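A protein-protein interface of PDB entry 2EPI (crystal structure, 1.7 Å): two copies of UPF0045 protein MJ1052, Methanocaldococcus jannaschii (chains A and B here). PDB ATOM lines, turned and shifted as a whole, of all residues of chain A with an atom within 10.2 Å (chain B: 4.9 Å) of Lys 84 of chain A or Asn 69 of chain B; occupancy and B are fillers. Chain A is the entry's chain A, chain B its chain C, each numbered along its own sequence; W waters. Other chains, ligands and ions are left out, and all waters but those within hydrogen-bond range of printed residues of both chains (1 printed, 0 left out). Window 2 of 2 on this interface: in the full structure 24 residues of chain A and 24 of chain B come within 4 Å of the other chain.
The guanidinium group of Arg 5 of chain A sits at hydrogen-bond distance from the side-chain hydroxyl of Ser 65 of chain B, at 2.9 Å. The side-chain amino group of Lys 84 of chain A sits at hydrogen-bond distance from the backbone carbonyl oxygen of Leu 68 of chain B, at 2.8 Å. The backbone carbonyl oxygen (O) of Asn 69 of chain B is in hydrogen-bond range of the side-chain amino group (NZ) of Lys 84 of chain A (3.4 Å). The side-chain amino group of Lys 84 of chain A lies close to the backbone carbonyl oxygen of Val 71 of chain B. O of Asp 72 of chain B lies within hydrogen-bond range of N of Lys 84 of chain A, at 2.8 Å.
The guanidinium group (NH2) of Arg 5 of chain A is in salt-bridge range of the side-chain carboxylate (OE1) of Glu 82 of chain A, at 2.9 Å. The guanidinium group (NH2) of Arg 83 of chain A lies within salt-bridge range of the side-chain carboxylate (OD2) of Asp 85 of chain A, at 2.7 Å. The backbone NH (N) of Arg 83 of chain A sits at hydrogen-bond distance from the side-chain amide oxygen (OD1) of Asn 88 of chain A (2.8 Å). The side-chain amide nitrogen (ND2) of Asn 69 of chain B is in hydrogen-bond range of the side-chain carboxylate (OD1) of Asp 70 of chain B (3.3 Å).
Arg 5 of chain A touches Leu 68 of chain B. Glu 82 of chain A touches Leu 68 of chain B. Asp 72 of chain B touches Arg 83 of chain A (O to CA, 3.0 Å). Asp 72 of chain B touches Asp 85 of chain A (O to OD1, 3.8 Å).
Of the printed residues of chain B, Lys 84 of chain A touches Leu 68, Asn 69, Val 71 and Asp 72. Of chain A, only Lys 84 (3.4 Å) comes within 4 Å of Asn 69 of chain B. Leu 68 of chain B touches just these residues of chain A: Arg 5 (3.9 Å), Glu 82 (3.2 Å) and Lys 84 (2.8 Å). No residue of chain A comes within 4 Å of Asp 70 of chain B. Of the printed residues of chain B, Glu 82 of chain A touches Leu 68. Printed residues of chain A within 4 Å of Val 71 of chain B: Lys 84 (2.9 Å). Of the printed residues of chain B, Arg 83 of chain A touches Asp 72 (3.0 Å). Printed residues of chain B within 4 Å of Arg 5 of chain A: Ser 65 and Leu 68. Arg 92 of chain A touches none of the printed residues of chain B. Asp 81 of chain A touches none of the printed residues of chain B. The nearest residue of chain B that does not touch Lys 84 of chain A is Asp 70 of chain B (4.6 Å).
Of the 8 printed residues of chain B, 5 touch a printed residue of chain A. Hydrophobic or aromatic side chains of chain B that line the printed part of chain A: Leu 68. Of the 13 printed residues of chain A, 5 touch a printed residue of chain B. Among the printed residues, 9 pairs touch across the chains. Among the printed residues, no Asp or Glu carboxylate lies within 4 Å of a Lys or Arg side-chain nitrogen of the other chain.
No position is printed for both chains.
Water W1 lies within hydrogen-bond range of OG of Ser 65 of chain B (3.3 Å) and NH1 of Arg 5 of chain A (3.4 Å).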
ATOM      1  N   ARG A   5     -17.546  15.081   0.916  1.00  0.00           N
ATOM      2  CA  ARG A   5     -18.401  14.723  -0.200  1.00  0.00           C
ATOM      3  C   ARG A   5     -17.391  14.121  -1.166  1.00  0.00           C
ATOM      4  O   ARG A   5     -16.887  14.800  -2.059  1.00  0.00           O
ATOM      5  CB  ARG A   5     -19.047  15.965  -0.812  1.00  0.00           C
ATOM      6  CG  ARG A   5     -19.885  15.659  -2.037  1.00  0.00           C
ATOM      7  CD  ARG A   5     -20.546  16.901  -2.599  1.00  0.00           C
ATOM      8  NE  ARG A   5     -21.168  16.620  -3.887  1.00  0.00           N
ATOM      9  CZ  ARG A   5     -21.838  17.511  -4.610  1.00  0.00           C
ATOM     10  NH1 ARG A   5     -21.981  18.758  -4.174  1.00  0.00           N
ATOM     11  NH2 ARG A   5     -22.357  17.151  -5.774  1.00  0.00           N
ATOM     12  N   LYS A   6     -17.087  12.844  -0.966  1.00  0.00           N
ATOM     13  CA  LYS A   6     -16.092  12.157  -1.776  1.00  0.00           C
ATOM     14  C   LYS A   6     -16.461  11.859  -3.226  1.00  0.00           C
ATOM     15  O   LYS A   6     -17.579  11.439  -3.539  1.00  0.00           O
ATOM     16  CB  LYS A   6     -15.669  10.860  -1.075  1.00  0.00           C
ATOM     17  CG  LYS A   6     -14.511  10.143  -1.752  1.00  0.00           C
ATOM     18  CD  LYS A   6     -14.047   8.931  -0.952  1.00  0.00           C
ATOM     19  CE  LYS A   6     -13.440   9.345   0.386  1.00  0.00           C
ATOM     20  NZ  LYS A   6     -12.921   8.169   1.142  1.00  0.00           N
ATOM     21  N   VAL A   7     -15.492  12.091  -4.108  1.00  0.00           N
ATOM     22  CA  VAL A   7     -15.643  11.841  -5.534  1.00  0.00           C
ATOM     23  C   VAL A   7     -14.292  11.408  -6.087  1.00  0.00           C
ATOM     24  O   VAL A   7     -13.270  11.531  -5.416  1.00  0.00           O
ATOM     25  CB  VAL A   7     -16.074  13.118  -6.310  1.00  0.00           C
ATOM     26  CG1 VAL A   7     -17.355  13.687  -5.720  1.00  0.00           C
ATOM     27  CG2 VAL A   7     -14.956  14.159  -6.271  1.00  0.00           C
ATOM     28  N   ASP A  81     -16.387  12.263 -11.228  1.00  0.00           N
ATOM     29  CA  ASP A  81     -17.243  11.084 -11.315  1.00  0.00           C
ATOM     30  C   ASP A  81     -17.792  10.897  -9.907  1.00  0.00           C
ATOM     31  O   ASP A  81     -17.055  10.526  -8.995  1.00  0.00           O
ATOM     32  CB  ASP A  81     -16.427   9.854 -11.720  1.00  0.00           C
ATOM     33  CG  ASP A  81     -17.299   8.651 -12.050  1.00  0.00           C
ATOM     34  OD1 ASP A  81     -18.413   8.542 -11.495  1.00  0.00           O
ATOM     35  OD2 ASP A  81     -16.863   7.803 -12.859  1.00  0.00           O
ATOM     36  N   GLU A  82     -19.080  11.168  -9.728  1.00  0.00           N
ATOM     37  CA  GLU A  82     -19.699  11.039  -8.414  1.00  0.00           C
ATOM     38  C   GLU A  82     -20.982  10.224  -8.452  1.00  0.00           C
ATOM     39  O   GLU A  82     -21.815  10.399  -9.339  1.00  0.00           O
ATOM     40  CB  GLU A  82     -19.994  12.429  -7.831  1.00  0.00           C
ATOM     41  CG  GLU A  82     -20.860  12.409  -6.568  1.00  0.00           C
ATOM     42  CD  GLU A  82     -20.977  13.769  -5.909  1.00  0.00           C
ATOM     43  OE1 GLU A  82     -20.951  14.785  -6.634  1.00  0.00           O
ATOM     44  OE2 GLU A  82     -21.109  13.824  -4.664  1.00  0.00           O
ATOM     45  N   ARG A  83     -21.132   9.327  -7.485  1.00  0.00           N
ATOM     46  CA  ARG A  83     -22.330   8.504  -7.403  1.00  0.00           C
ATOM     47  C   ARG A  83     -22.801   8.479  -5.954  1.00  0.00           C
ATOM     48  O   ARG A  83     -22.009   8.680  -5.030  1.00  0.00           O
ATOM     49  CB  ARG A  83     -22.051   7.086  -7.918  1.00  0.00           C
ATOM     50  CG  ARG A  83     -21.057   6.281  -7.098  1.00  0.00           C
ATOM     51  CD  ARG A  83     -20.687   4.990  -7.816  1.00  0.00           C
ATOM     52  NE  ARG A  83     -21.850   4.158  -8.118  1.00  0.00           N
ATOM     53  CZ  ARG A  83     -21.798   3.038  -8.835  1.00  0.00           C
ATOM     54  NH1 ARG A  83     -20.640   2.617  -9.325  1.00  0.00           N
ATOM     55  NH2 ARG A  83     -22.903   2.337  -9.062  1.00  0.00           N
ATOM     56  N   LYS A  84     -24.095   8.244  -5.758  1.00  0.00           N
ATOM     57  CA  LYS A  84     -24.667   8.224  -4.416  1.00  0.00           C
ATOM     58  C   LYS A  84     -25.071   6.825  -3.955  1.00  0.00           C
ATOM     59  O   LYS A  84     -25.368   6.618  -2.779  1.00  0.00           O
ATOM     60  CB  LYS A  84     -25.887   9.149  -4.369  1.00  0.00           C
ATOM     61  CG  LYS A  84     -27.062   8.640  -5.192  1.00  0.00           C
ATOM     62  CD  LYS A  84     -27.799   9.765  -5.901  1.00  0.00           C
ATOM     63  CE  LYS A  84     -28.481  10.711  -4.936  1.00  0.00           C
ATOM     64  NZ  LYS A  84     -29.274  11.724  -5.682  1.00  0.00           N
ATOM     65  N   ASP A  85     -25.072   5.865  -4.877  1.00  0.00           N
ATOM     66  CA  ASP A  85     -25.461   4.497  -4.549  1.00  0.00           C
ATOM     67  C   ASP A  85     -24.298   3.638  -4.064  1.00  0.00           C
ATOM     68  O   ASP A  85     -24.508   2.564  -3.503  1.00  0.00           O
ATOM     69  CB  ASP A  85     -26.114   3.832  -5.762  1.00  0.00           C
ATOM     70  CG  ASP A  85     -25.142   3.628  -6.909  1.00  0.00           C
ATOM     71  OD1 ASP A  85     -24.525   4.621  -7.352  1.00  0.00           O
ATOM     72  OD2 ASP A  85     -24.995   2.475  -7.367  1.00  0.00           O
ATOM     73  N   LYS A  86     -23.074   4.104  -4.288  1.00  0.00           N
ATOM     74  CA  LYS A  86     -21.892   3.362  -3.867  1.00  0.00           C
ATOM     75  C   LYS A  86     -20.761   4.296  -3.454  1.00  0.00           C
ATOM     76  O   LYS A  86     -20.803   5.499  -3.712  1.00  0.00           O
ATOM     77  CB  LYS A  86     -21.404   2.443  -4.991  1.00  0.00           C
ATOM     78  CG  LYS A  86     -22.390   1.358  -5.389  1.00  0.00           C
ATOM     79  CD  LYS A  86     -21.838   0.508  -6.522  1.00  0.00           C
ATOM     80  CE  LYS A  86     -22.841  -0.541  -6.971  1.00  0.00           C
ATOM     81  NZ  LYS A  86     -22.331  -1.325  -8.130  1.00  0.00           N
ATOM     82  N   GLU A  87     -19.751   3.723  -2.812  1.00  0.00           N
ATOM     83  CA  GLU A  87     -18.593   4.473  -2.347  1.00  0.00           C
ATOM     84  C   GLU A  87     -17.826   5.054  -3.532  1.00  0.00           C
ATOM     85  O   GLU A  87     -17.656   4.392  -4.553  1.00  0.00           O
ATOM     86  CB  GLU A  87     -17.691   3.548  -1.531  1.00  0.00           C
ATOM     87  CG  GLU A  87     -16.559   4.237  -0.803  1.00  0.00           C
ATOM     88  CD  GLU A  87     -15.908   3.327   0.223  1.00  0.00           C
ATOM     89  OE1 GLU A  87     -15.396   2.255  -0.168  1.00  0.00           O
ATOM     90  OE2 GLU A  87     -15.914   3.682   1.422  1.00  0.00           O
ATOM     91  N   ASN A  88     -17.370   6.295  -3.389  1.00  0.00           N
ATOM     92  CA  ASN A  88     -16.629   6.983  -4.447  1.00  0.00           C
ATOM     93  C   ASN A  88     -15.124   6.910  -4.209  1.00  0.00           C
ATOM     94  O   ASN A  88     -14.504   7.904  -3.841  1.00  0.00           O
ATOM     95  CB  ASN A  88     -17.058   8.454  -4.510  1.00  0.00           C
ATOM     96  CG  ASN A  88     -18.496   8.625  -4.967  1.00  0.00           C
ATOM     97  OD1 ASN A  88     -18.814   8.424  -6.140  1.00  0.00           O
ATOM     98  ND2 ASN A  88     -19.376   8.986  -4.037  1.00  0.00           N
ATOM     99  N   THR A  89     -14.535   5.739  -4.423  1.00  0.00           N
ATOM    100  CA  THR A  89     -13.099   5.587  -4.218  1.00  0.00           C
ATOM    101  C   THR A  89     -12.412   4.970  -5.424  1.00  0.00           C
ATOM    102  O   THR A  89     -13.039   4.286  -6.233  1.00  0.00           O
ATOM    103  CB  THR A  89     -12.788   4.693  -3.002  1.00  0.00           C
ATOM    104  OG1 THR A  89     -13.275   3.367  -3.250  1.00  0.00           O
ATOM    105  CG2 THR A  89     -13.452   5.244  -1.753  1.00  0.00           C
ATOM    106  N   ARG A  92     -12.537   1.010  -5.093  1.00  0.00           N
ATOM    107  CA  ARG A  92     -13.744   0.350  -5.567  1.00  0.00           C
ATOM    108  C   ARG A  92     -13.833   0.359  -7.089  1.00  0.00           C
ATOM    109  O   ARG A  92     -14.236  -0.632  -7.695  1.00  0.00           O
ATOM    110  CB  ARG A  92     -14.993   1.012  -4.981  1.00  0.00           C
ATOM    111  CG  ARG A  92     -16.266   0.218  -5.242  1.00  0.00           C
ATOM    112  CD  ARG A  92     -17.505   1.033  -4.923  1.00  0.00           C
ATOM    113  NE  ARG A  92     -17.613   2.205  -5.787  1.00  0.00           N
ATOM    114  CZ  ARG A  92     -17.786   2.151  -7.104  1.00  0.00           C
ATOM    115  NH1 ARG A  92     -17.878   0.978  -7.719  1.00  0.00           N
ATOM    116  NH2 ARG A  92     -17.863   3.273  -7.810  1.00  0.00           N
ATOM    117  N   SER B  65     -24.230  19.122  -9.269  1.00  0.00           N
ATOM    118  CA  SER B  65     -25.045  18.735  -8.124  1.00  0.00           C
ATOM    119  C   SER B  65     -26.539  18.667  -8.421  1.00  0.00           C
ATOM    120  O   SER B  65     -27.221  17.739  -7.986  1.00  0.00           O
ATOM    121  CB  SER B  65     -24.804  19.705  -6.968  1.00  0.00           C
ATOM    122  OG  SER B  65     -23.449  19.686  -6.565  1.00  0.00           O
ATOM    123  N   THR B  66     -27.048  19.650  -9.155  1.00  0.00           N
ATOM    124  CA  THR B  66     -28.467  19.675  -9.479  1.00  0.00           C
ATOM    125  C   THR B  66     -28.867  18.456 -10.309  1.00  0.00           C
ATOM    126  O   THR B  66     -29.965  17.930 -10.152  1.00  0.00           O
ATOM    127  CB  THR B  66     -28.848  20.966 -10.234  1.00  0.00           C
ATOM    128  OG1 THR B  66     -30.272  21.022 -10.394  1.00  0.00           O
ATOM    129  CG2 THR B  66     -28.194  21.003 -11.595  1.00  0.00           C
ATOM    130  N   VAL B  67     -27.980  18.002 -11.190  1.00  0.00           N
ATOM    131  CA  VAL B  67     -28.279  16.829 -12.004  1.00  0.00           C
ATOM    132  C   VAL B  67     -28.165  15.572 -11.147  1.00  0.00           C
ATOM    133  O   VAL B  67     -28.945  14.630 -11.297  1.00  0.00           O
ATOM    134  CB  VAL B  67     -27.313  16.703 -13.209  1.00  0.00           C
ATOM    135  CG1 VAL B  67     -27.544  15.380 -13.932  1.00  0.00           C
ATOM    136  CG2 VAL B  67     -27.530  17.859 -14.171  1.00  0.00           C
ATOM    137  N   LEU B  68     -27.198  15.568 -10.238  1.00  0.00           N
ATOM    138  CA  LEU B  68     -26.981  14.428  -9.358  1.00  0.00           C
ATOM    139  C   LEU B  68     -28.142  14.258  -8.383  1.00  0.00           C
ATOM    140  O   LEU B  68     -28.403  13.160  -7.896  1.00  0.00           O
ATOM    141  CB  LEU B  68     -25.675  14.598  -8.577  1.00  0.00           C
ATOM    142  CG  LEU B  68     -25.345  13.496  -7.565  1.00  0.00           C
ATOM    143  CD1 LEU B  68     -25.333  12.141  -8.250  1.00  0.00           C
ATOM    144  CD2 LEU B  68     -24.002  13.783  -6.923  1.00  0.00           C
ATOM    145  N   ASN B  69     -28.842  15.349  -8.104  1.00  0.00           N
ATOM    146  CA  ASN B  69     -29.967  15.300  -7.182  1.00  0.00           C
ATOM    147  C   ASN B  69     -31.056  14.353  -7.690  1.00  0.00           C
ATOM    148  O   ASN B  69     -31.773  13.744  -6.897  1.00  0.00           O
ATOM    149  CB  ASN B  69     -30.548  16.704  -6.989  1.00  0.00           C
ATOM    150  CG  ASN B  69     -31.683  16.732  -5.981  1.00  0.00           C
ATOM    151  OD1 ASN B  69     -31.490  16.424  -4.805  1.00  0.00           O
ATOM    152  ND2 ASN B  69     -32.875  17.101  -6.440  1.00  0.00           N
ATOM    153  N   ASP B  70     -31.167  14.220  -9.011  1.00  0.00           N
ATOM    154  CA  ASP B  70     -32.189  13.365  -9.606  1.00  0.00           C
ATOM    155  C   ASP B  70     -31.725  11.978 -10.047  1.00  0.00           C
ATOM    156  O   ASP B  70     -32.549  11.106 -10.324  1.00  0.00           O
ATOM    157  CB  ASP B  70     -32.834  14.074 -10.802  1.00  0.00           C
ATOM    158  CG  ASP B  70     -33.308  15.474 -10.465  1.00  0.00           C
ATOM    159  OD1 ASP B  70     -33.703  15.707  -9.302  1.00  0.00           O
ATOM    160  OD2 ASP B  70     -33.297  16.339 -11.366  1.00  0.00           O
ATOM    161  N   VAL B  71     -30.416  11.766 -10.124  1.00  0.00           N
ATOM    162  CA  VAL B  71     -29.902  10.468 -10.546  1.00  0.00           C
ATOM    163  C   VAL B  71     -28.890   9.899  -9.556  1.00  0.00           C
ATOM    164  O   VAL B  71     -28.528  10.557  -8.583  1.00  0.00           O
ATOM    165  CB  VAL B  71     -29.257  10.562 -11.941  1.00  0.00           C
ATOM    166  CG1 VAL B  71     -30.275  11.082 -12.939  1.00  0.00           C
ATOM    167  CG2 VAL B  71     -28.040  11.473 -11.896  1.00  0.00           C
ATOM    168  N   ASP B  72     -28.434   8.674  -9.809  1.00  0.00           N
ATOM    169  CA  ASP B  72     -27.479   8.014  -8.925  1.00  0.00           C
ATOM    170  C   ASP B  72     -26.017   8.328  -9.215  1.00  0.00           C
ATOM    171  O   ASP B  72     -25.181   8.279  -8.316  1.00  0.00           O
ATOM    172  CB  ASP B  72     -27.660   6.494  -8.980  1.00  0.00           C
ATOM    173  CG  ASP B  72     -28.963   6.034  -8.358  1.00  0.00           C
ATOM    174  OD1 ASP B  72     -29.295   6.515  -7.256  1.00  0.00           O
ATOM    175  OD2 ASP B  72     -29.644   5.184  -8.968  1.00  0.00           O
HETATM  176  O   HOH W   1     -23.915  21.480  -3.791  1.00  0.00           O
